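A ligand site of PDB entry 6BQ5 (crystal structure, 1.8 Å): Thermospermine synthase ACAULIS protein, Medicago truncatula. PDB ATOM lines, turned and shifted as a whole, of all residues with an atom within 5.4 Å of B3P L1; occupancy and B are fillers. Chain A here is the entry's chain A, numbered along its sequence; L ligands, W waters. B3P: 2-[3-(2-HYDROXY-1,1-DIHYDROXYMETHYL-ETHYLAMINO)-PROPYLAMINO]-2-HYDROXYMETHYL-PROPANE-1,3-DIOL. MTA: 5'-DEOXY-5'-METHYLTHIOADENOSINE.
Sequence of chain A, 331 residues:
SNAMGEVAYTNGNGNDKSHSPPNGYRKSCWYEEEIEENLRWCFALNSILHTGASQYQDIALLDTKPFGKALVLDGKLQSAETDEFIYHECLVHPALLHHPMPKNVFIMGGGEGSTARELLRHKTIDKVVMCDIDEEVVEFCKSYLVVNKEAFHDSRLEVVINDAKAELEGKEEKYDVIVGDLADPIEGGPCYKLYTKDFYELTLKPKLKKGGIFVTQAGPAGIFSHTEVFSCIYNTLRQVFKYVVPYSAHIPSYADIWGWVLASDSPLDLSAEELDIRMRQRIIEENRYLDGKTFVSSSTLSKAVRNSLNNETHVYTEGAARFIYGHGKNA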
ATOM      1  N   GLU A  33     -18.918 -10.120   5.898  1.00  0.00           N
ATOM      2  CA  GLU A  33     -18.512 -10.156   4.528  1.00  0.00           C
ATOM      3  C   GLU A  33     -17.201 -10.909   4.411  1.00  0.00           C
ATOM      4  O   GLU A  33     -16.309 -10.711   5.217  1.00  0.00           O
ATOM      5  CB  GLU A  33     -18.422  -8.740   3.957  1.00  0.00           C
ATOM      6  CG  GLU A  33     -18.035  -8.810   2.503  1.00  0.00           C
ATOM      7  CD  GLU A  33     -17.990  -7.494   1.777  1.00  0.00           C
ATOM      8  OE1 GLU A  33     -18.478  -6.454   2.335  1.00  0.00           O
ATOM      9  OE2 GLU A  33     -17.435  -7.495   0.673  1.00  0.00           O
ATOM     10  N   ILE A  35     -14.125 -10.803   2.912  1.00  0.00           N
ATOM     11  CA  ILE A  35     -13.453  -9.796   2.099  1.00  0.00           C
ATOM     12  C   ILE A  35     -12.249 -10.367   1.346  1.00  0.00           C
ATOM     13  O   ILE A  35     -11.707  -9.749   0.474  1.00  0.00           O
ATOM     14  CB  ILE A  35     -13.077  -8.502   2.880  1.00  0.00           C
ATOM     15  CG1 ILE A  35     -12.134  -8.798   4.024  1.00  0.00           C
ATOM     16  CG2 ILE A  35     -14.332  -7.801   3.394  1.00  0.00           C
ATOM     17  CD1 ILE A  35     -11.569  -7.533   4.660  1.00  0.00           C
ATOM     18  N   GLY A  75     -23.739  -7.306  -2.027  1.00  0.00           N
ATOM     19  CA  GLY A  75     -23.124  -7.904  -0.832  1.00  0.00           C
ATOM     20  C   GLY A  75     -21.679  -7.501  -0.562  1.00  0.00           C
ATOM     21  O   GLY A  75     -20.951  -8.202   0.190  1.00  0.00           O
ATOM     22  N   LYS A  76     -21.275  -6.376  -1.158  1.00  0.00           N
ATOM     23  CA  LYS A  76     -19.921  -5.827  -1.007  1.00  0.00           C
ATOM     24  C   LYS A  76     -20.023  -4.435  -0.500  1.00  0.00           C
ATOM     25  O   LYS A  76     -20.728  -3.609  -1.074  1.00  0.00           O
ATOM     26  CB  LYS A  76     -19.186  -5.835  -2.337  1.00  0.00           C
ATOM     27  CG  LYS A  76     -19.131  -7.210  -2.973  1.00  0.00           C
ATOM     28  CD  LYS A  76     -18.115  -7.306  -4.096  1.00  0.00           C
ATOM     29  CE  LYS A  76     -16.764  -7.863  -3.631  1.00  0.00           C
ATOM     30  NZ  LYS A  76     -15.534  -7.572  -4.499  1.00  0.00           N
ATOM     31  N   LEU A  77     -19.334  -4.157   0.607  1.00  0.00           N
ATOM     32  CA  LEU A  77     -19.335  -2.827   1.201  1.00  0.00           C
ATOM     33  C   LEU A  77     -18.762  -1.827   0.204  1.00  0.00           C
ATOM     34  O   LEU A  77     -17.693  -2.071  -0.351  1.00  0.00           O
ATOM     35  CB  LEU A  77     -18.472  -2.809   2.452  1.00  0.00           C
ATOM     36  CG  LEU A  77     -18.257  -1.484   3.124  1.00  0.00           C
ATOM     37  CD1 LEU A  77     -19.550  -1.059   3.817  1.00  0.00           C
ATOM     38  CD2 LEU A  77     -17.117  -1.630   4.127  1.00  0.00           C
ATOM     39  N   GLN A  78     -19.479  -0.719   0.021  1.00  0.00           N
ATOM     40  CA  GLN A  78     -19.005   0.420  -0.820  1.00  0.00           C
ATOM     41  C   GLN A  78     -18.529   1.627  -0.011  1.00  0.00           C
ATOM     42  O   GLN A  78     -17.376   2.012  -0.121  1.00  0.00           O
ATOM     43  CB  GLN A  78     -20.086   0.857  -1.776  1.00  0.00           C
ATOM     44  CG  GLN A  78     -20.643  -0.288  -2.637  1.00  0.00           C
ATOM     45  CD  GLN A  78     -19.593  -0.882  -3.554  1.00  0.00           C
ATOM     46  OE1 GLN A  78     -18.925  -0.154  -4.260  1.00  0.00           O
ATOM     47  NE2 GLN A  78     -19.417  -2.206  -3.534  1.00  0.00           N
ATOM     48  N   SER A  79     -19.410   2.203   0.783  1.00  0.00           N
ATOM     49  CA  SER A  79     -19.159   3.445   1.474  1.00  0.00           C
ATOM     50  C   SER A  79     -19.757   3.325   2.860  1.00  0.00           C
ATOM     51  O   SER A  79     -20.914   2.936   2.986  1.00  0.00           O
ATOM     52  CB  SER A  79     -19.822   4.600   0.703  1.00  0.00           C
ATOM     53  OG  SER A  79     -18.979   5.007  -0.395  1.00  0.00           O
ATOM     54  N   TYR A  87     -11.827   7.994   1.389  1.00  0.00           N
ATOM     55  CA  TYR A  87     -11.848   7.583   0.007  1.00  0.00           C
ATOM     56  C   TYR A  87     -12.192   8.754  -0.892  1.00  0.00           C
ATOM     57  O   TYR A  87     -11.520   8.979  -1.878  1.00  0.00           O
ATOM     58  CB  TYR A  87     -12.825   6.414  -0.223  1.00  0.00           C
ATOM     59  CG  TYR A  87     -13.031   6.047  -1.663  1.00  0.00           C
ATOM     60  CD1 TYR A  87     -13.980   6.711  -2.418  1.00  0.00           C
ATOM     61  CD2 TYR A  87     -12.282   5.049  -2.292  1.00  0.00           C
ATOM     62  CE1 TYR A  87     -14.185   6.425  -3.789  1.00  0.00           C
ATOM     63  CE2 TYR A  87     -12.508   4.723  -3.639  1.00  0.00           C
ATOM     64  CZ  TYR A  87     -13.426   5.426  -4.373  1.00  0.00           C
ATOM     65  OH  TYR A  87     -13.660   5.168  -5.699  1.00  0.00           O
ATOM     66  N   ASP A 181     -14.752   6.391 -10.798  1.00  0.00           N
ATOM     67  CA  ASP A 181     -15.298   5.956  -9.509  1.00  0.00           C
ATOM     68  C   ASP A 181     -16.054   4.648  -9.718  1.00  0.00           C
ATOM     69  O   ASP A 181     -17.157   4.441  -9.172  1.00  0.00           O
ATOM     70  CB  ASP A 181     -16.186   7.064  -8.950  1.00  0.00           C
ATOM     71  CG  ASP A 181     -16.566   6.920  -7.465  1.00  0.00           C
ATOM     72  OD1 ASP A 181     -15.987   6.055  -6.736  1.00  0.00           O
ATOM     73  OD2 ASP A 181     -17.440   7.714  -7.036  1.00  0.00           O
ATOM     74  N   LEU A 182     -15.431   3.745 -10.460  1.00  0.00           N
ATOM     75  CA  LEU A 182     -16.027   2.467 -10.817  1.00  0.00           C
ATOM     76  C   LEU A 182     -15.551   1.324  -9.933  1.00  0.00           C
ATOM     77  O   LEU A 182     -14.686   1.500  -9.041  1.00  0.00           O
ATOM     78  CB  LEU A 182     -15.702   2.148 -12.282  1.00  0.00           C
ATOM     79  CG  LEU A 182     -16.206   3.139 -13.319  1.00  0.00           C
ATOM     80  CD1 LEU A 182     -15.423   3.077 -14.635  1.00  0.00           C
ATOM     81  CD2 LEU A 182     -17.683   2.996 -13.589  1.00  0.00           C
ATOM     82  N   ALA A 183     -16.123   0.131 -10.172  1.00  0.00           N
ATOM     83  CA  ALA A 183     -15.614  -1.103  -9.659  1.00  0.00           C
ATOM     84  C   ALA A 183     -14.256  -1.442 -10.284  1.00  0.00           C
ATOM     85  O   ALA A 183     -13.858  -0.929 -11.307  1.00  0.00           O
ATOM     86  CB  ALA A 183     -16.606  -2.277  -9.863  1.00  0.00           C
ATOM     87  N   ASP A 184     -13.546  -2.284  -9.584  1.00  0.00           N
ATOM     88  CA  ASP A 184     -12.274  -2.863 -10.062  1.00  0.00           C
ATOM     89  C   ASP A 184     -12.388  -3.577 -11.424  1.00  0.00           C
ATOM     90  O   ASP A 184     -13.391  -4.234 -11.661  1.00  0.00           O
ATOM     91  CB  ASP A 184     -11.756  -3.877  -9.055  1.00  0.00           C
ATOM     92  CG  ASP A 184     -11.094  -3.258  -7.841  1.00  0.00           C
ATOM     93  OD1 ASP A 184     -10.991  -2.022  -7.774  1.00  0.00           O
ATOM     94  OD2 ASP A 184     -10.655  -4.019  -6.955  1.00  0.00           O
ATOM     95  N   GLN A 217      -9.910   5.675  -9.076  1.00  0.00           N
ATOM     96  CA  GLN A 217      -9.751   4.625  -8.059  1.00  0.00           C
ATOM     97  C   GLN A 217      -9.031   3.419  -8.731  1.00  0.00           C
ATOM     98  O   GLN A 217      -9.216   3.117  -9.895  1.00  0.00           O
ATOM     99  CB  GLN A 217     -11.074   4.221  -7.427  1.00  0.00           C
ATOM    100  CG  GLN A 217     -11.854   3.144  -8.201  1.00  0.00           C
ATOM    101  CD  GLN A 217     -11.408   1.717  -7.846  1.00  0.00           C
ATOM    102  OE1 GLN A 217     -11.026   1.427  -6.693  1.00  0.00           O
ATOM    103  NE2 GLN A 217     -11.455   0.842  -8.802  1.00  0.00           N
ATOM    104  N   PRO A 220      -7.329  -2.273  -4.321  1.00  0.00           N
ATOM    105  CA  PRO A 220      -6.552  -2.470  -3.105  1.00  0.00           C
ATOM    106  C   PRO A 220      -5.077  -2.154  -3.351  1.00  0.00           C
ATOM    107  O   PRO A 220      -4.573  -2.380  -4.482  1.00  0.00           O
ATOM    108  CB  PRO A 220      -6.689  -3.954  -2.831  1.00  0.00           C
ATOM    109  CG  PRO A 220      -7.899  -4.382  -3.553  1.00  0.00           C
ATOM    110  CD  PRO A 220      -8.008  -3.500  -4.756  1.00  0.00           C
ATOM    111  N   SER A 253     -12.774   0.811   7.142  1.00  0.00           N
ATOM    112  CA  SER A 253     -13.924  -0.042   6.899  1.00  0.00           C
ATOM    113  C   SER A 253     -13.651  -1.120   5.862  1.00  0.00           C
ATOM    114  O   SER A 253     -14.371  -2.149   5.813  1.00  0.00           O
ATOM    115  CB  SER A 253     -15.188   0.759   6.540  1.00  0.00           C
ATOM    116  OG  SER A 253     -15.011   1.485   5.364  1.00  0.00           O
ATOM    117  N   TYR A 254     -12.651  -0.886   5.022  1.00  0.00           N
ATOM    118  CA  TYR A 254     -12.186  -1.884   4.037  1.00  0.00           C
ATOM    119  C   TYR A 254     -11.132  -2.835   4.575  1.00  0.00           C
ATOM    120  O   TYR A 254     -10.754  -3.771   3.892  1.00  0.00           O
ATOM    121  CB  TYR A 254     -11.561  -1.174   2.882  1.00  0.00           C
ATOM    122  CG  TYR A 254     -12.446  -0.388   2.001  1.00  0.00           C
ATOM    123  CD1 TYR A 254     -13.796  -0.184   2.296  1.00  0.00           C
ATOM    124  CD2 TYR A 254     -11.950   0.153   0.844  1.00  0.00           C
ATOM    125  CE1 TYR A 254     -14.592   0.560   1.437  1.00  0.00           C
ATOM    126  CE2 TYR A 254     -12.724   0.891  -0.023  1.00  0.00           C
ATOM    127  CZ  TYR A 254     -14.045   1.101   0.275  1.00  0.00           C
ATOM    128  OH  TYR A 254     -14.842   1.879  -0.536  1.00  0.00           O
ATOM    129  N   ALA A 255     -10.654  -2.621   5.786  1.00  0.00           N
ATOM    130  CA  ALA A 255      -9.522  -3.412   6.342  1.00  0.00           C
ATOM    131  C   ALA A 255      -8.363  -3.580   5.321  1.00  0.00           C
ATOM    132  O   ALA A 255      -7.656  -4.620   5.285  1.00  0.00           O
ATOM    133  CB  ALA A 255      -9.951  -4.778   6.883  1.00  0.00           C
ATOM    134  N   TRP A 258      -6.211   1.413   0.220  1.00  0.00           N
ATOM    135  CA  TRP A 258      -6.757   1.594  -1.066  1.00  0.00           C
ATOM    136  C   TRP A 258      -5.893   2.519  -1.929  1.00  0.00           C
ATOM    137  O   TRP A 258      -5.216   3.424  -1.423  1.00  0.00           O
ATOM    138  CB  TRP A 258      -8.176   2.153  -0.974  1.00  0.00           C
ATOM    139  CG  TRP A 258      -9.038   1.724  -2.055  1.00  0.00           C
ATOM    140  CD1 TRP A 258      -9.415   2.424  -3.129  1.00  0.00           C
ATOM    141  CD2 TRP A 258      -9.596   0.433  -2.192  1.00  0.00           C
ATOM    142  NE1 TRP A 258     -10.217   1.682  -3.922  1.00  0.00           N
ATOM    143  CE2 TRP A 258     -10.348   0.443  -3.374  1.00  0.00           C
ATOM    144  CE3 TRP A 258      -9.548  -0.721  -1.420  1.00  0.00           C
ATOM    145  CZ2 TRP A 258     -10.995  -0.682  -3.856  1.00  0.00           C
ATOM    146  CZ3 TRP A 258     -10.245  -1.836  -1.871  1.00  0.00           C
ATOM    147  CH2 TRP A 258     -10.959  -1.801  -3.081  1.00  0.00           C
HETATM  148  C1  B3P L   1     -15.763  -1.588  -3.056  1.00  0.00           C
HETATM  149  C2  B3P L   1     -14.870  -2.094  -1.937  1.00  0.00           C
HETATM  150  C3  B3P L   1     -15.198  -0.242  -3.505  1.00  0.00           C
HETATM  151  N1  B3P L   1     -16.068   0.435  -4.461  1.00  0.00           N
HETATM  152  C4  B3P L   1     -15.745   1.767  -4.956  1.00  0.00           C
HETATM  153  C5  B3P L   1     -16.866   2.121  -5.961  1.00  0.00           C
HETATM  154  C6  B3P L   1     -15.683   2.747  -3.791  1.00  0.00           C
HETATM  155  C7  B3P L   1     -14.366   1.759  -5.627  1.00  0.00           C
HETATM  156  N2  B3P L   1     -15.257  -3.420  -1.505  1.00  0.00           N
HETATM  157  C8  B3P L   1     -14.465  -4.178  -0.565  1.00  0.00           C
HETATM  158  C9  B3P L   1     -15.223  -5.495  -0.371  1.00  0.00           C
HETATM  159  C10 B3P L   1     -14.308  -3.385   0.750  1.00  0.00           C
HETATM  160  C11 B3P L   1     -13.078  -4.500  -1.131  1.00  0.00           C
HETATM  161  O1  B3P L   1     -16.579  -5.213  -0.028  1.00  0.00           O
HETATM  162  O2  B3P L   1     -13.597  -4.185   1.698  1.00  0.00           O
HETATM  163  O3  B3P L   1     -13.139  -4.867  -2.510  1.00  0.00           O
HETATM  164  O4  B3P L   1     -16.642   3.383  -6.572  1.00  0.00           O
HETATM  165  O5  B3P L   1     -16.775   2.541  -2.891  1.00  0.00           O
HETATM  166  O6  B3P L   1     -14.211   0.738  -6.641  1.00  0.00           O
HETATM  167  CS  MTA L   2     -19.730  -0.329  -7.233  1.00  0.00           C
HETATM  168  S5' MTA L   2     -19.510   0.140  -8.902  1.00  0.00           S
HETATM  169  C5' MTA L   2     -19.502   1.886  -8.662  1.00  0.00           C
HETATM  170  C4' MTA L   2     -20.568   2.540  -9.546  1.00  0.00           C
HETATM  171  O4' MTA L   2     -20.267   2.320 -10.915  1.00  0.00           O
HETATM  172  C2' MTA L   2     -22.383   1.392 -10.651  1.00  0.00           C
HETATM  173  O2' MTA L   2     -23.777   1.604 -10.867  1.00  0.00           O
HETATM  174  C3' MTA L   2     -21.967   1.962  -9.327  1.00  0.00           C
HETATM  175  O3' MTA L   2     -22.804   3.002  -8.840  1.00  0.00           O
HETATM  176  C1' MTA L   2     -21.519   2.169 -11.612  1.00  0.00           C
HETATM  177  N9  MTA L   2     -21.124   1.570 -12.885  1.00  0.00           N
HETATM  178  C8  MTA L   2     -20.755   0.308 -13.155  1.00  0.00           C
HETATM  179  N7  MTA L   2     -20.400   0.182 -14.458  1.00  0.00           N
HETATM  180  C5  MTA L   2     -20.531   1.400 -15.011  1.00  0.00           C
HETATM  181  C6  MTA L   2     -20.343   1.954 -16.353  1.00  0.00           C
HETATM  182  N6  MTA L   2     -19.902   1.170 -17.368  1.00  0.00           N
HETATM  183  N1  MTA L   2     -20.574   3.268 -16.515  1.00  0.00           N
HETATM  184  C2  MTA L   2     -21.015   4.052 -15.500  1.00  0.00           C
HETATM  185  N3  MTA L   2     -21.216   3.615 -14.244  1.00  0.00           N
HETATM  186  C4  MTA L   2     -21.004   2.304 -13.983  1.00  0.00           C
HETATM  187  O   HOH W   1     -19.059   4.183  -3.261  1.00  0.00           O
HETATM  188  O   HOH W   2     -16.341   4.570  -0.855  1.00  0.00           O
HETATM  189  O   HOH W   3     -15.864  -4.869  -3.822  1.00  0.00           O
HETATM  190  O   HOH W   4     -10.384  -6.533  -2.314  1.00  0.00           O
HETATM  191  O   HOH W   5     -11.014  -5.026   1.607  1.00  0.00           O
HETATM  192  O   HOH W   6     -11.377  -5.001  -4.561  1.00  0.00           O
HETATM  193  O   HOH W   7     -19.215   5.110  -7.411  1.00  0.00           O
HETATM  194  O   HOH W   8     -14.916  -4.104   3.823  1.00  0.00           O
HETATM  195  O   HOH W   9     -13.561  -3.673  -4.881  1.00  0.00           O
HETATM  196  O   HOH W  10     -16.642  -1.414  -6.283  1.00  0.00           O
HETATM  197  O   HOH W  11     -13.350  -7.814  -1.325  1.00  0.00           O
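OE2 of Glu 33 is in hydrogen-bond range of O1 of B3P L1 (2.5 Å).
The backbone carbonyl oxygen (O) of Leu 182 sits at hydrogen-bond distance from an oxygen (O6) of B3P L1 (2.6 Å).
The backbone carbonyl oxygen of Asp 181 lies within hydrogen-bond range of an oxygen (O4) of B3P L1 (2.9 Å).
O4 of B3P L1 is in hydrogen-bond range of OD1 of Asp 181.
O5 of B3P L1 is in hydrogen-bond range of O of Gln 78 (2.9 Å).
The side-chain amide oxygen (OE1) of Gln 78 is in hydrogen-bond range of a nitrogen (N1) of B3P L1 (2.9 Å).
The backbone NH of Leu 77 sits at hydrogen-bond distance from an oxygen (O1) of B3P L1 (3.0 Å).
A nitrogen (N2) of B3P L1 sits at hydrogen-bond distance from the backbone carbonyl oxygen (O) of Leu 77 (3.0 Å).
The side-chain hydroxyl (OH) of Tyr 254 is in hydrogen-bond range of an oxygen (O5) of B3P L1, at 3.1 Å.
The side-chain amide oxygen (OE1) of Gln 217 sits close to an oxygen (O6) of B3P L1, at 3.3 Å.
The backbone NH of Ala 183 lies close to a sulfur (S5') of MTA L2 (3.6 Å).
The side-chain carboxylate (OE1) of Glu 33 lies within hydrogen-bond range of the backbone NH (N) of Leu 77 (3.0 Å).
NE2 of Gln 217 lies within hydrogen-bond range of O of Leu 182, at 3.3 Å.
OD1 of Asp 181 lies within hydrogen-bond range of OH of Tyr 87 (2.7 Å).
The backbone carbonyl oxygen (O) of Gln 78 lies within hydrogen-bond range of the side-chain hydroxyl (OH) of Tyr 254.
O of Lys 76 lies within hydrogen-bond range of NE2 of Gln 78, at 3.1 Å.
The side-chain amide oxygen (OE1) of Gln 217 sits at hydrogen-bond distance from the indole nitrogen (NE1) of Trp 258 (2.9 Å).
The side-chain carboxylate of Asp 184 sits at hydrogen-bond distance from the side-chain amide nitrogen of Gln 217 (3.1 Å).
Residues that only touch B3P L1: Tyr 87 (3.5 Å), Lys 76 (3.5 Å), Ala 183 (3.8 Å) and Trp 258 (3.8 Å).
Hydrophobic or aromatic side chains that line B3P L1: Leu 77, Tyr 87, Tyr 254 and Trp 258.
Water W8 lies within hydrogen-bond range of O2 of B3P L1 (2.5 Å) and O of Ser 253 (2.8 Å).
Water W6 lies within hydrogen-bond range of the side-chain carboxylate (OD2) of Asp 184 (2.7 Å) and an oxygen (O3) of B3P L1 (2.7 Å).
Water W5 bridges O of Tyr 254 and O2 of B3P L1.
Water W3 lies within hydrogen-bond range of a nitrogen (N2) of B3P L1 (2.8 Å) and the side-chain amino group (NZ) of Lys 76 (2.8 Å).
Water W2 lies within hydrogen-bond range of the side-chain hydroxyl of Ser 79, the backbone carbonyl oxygen of Gln 78, an oxygen (O5) of B3P L1 and the side-chain hydroxyl of Tyr 254.
Water W11 lies within hydrogen-bond range of O of Ile 35 (3.1 Å) and O3 of B3P L1 (3.2 Å).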
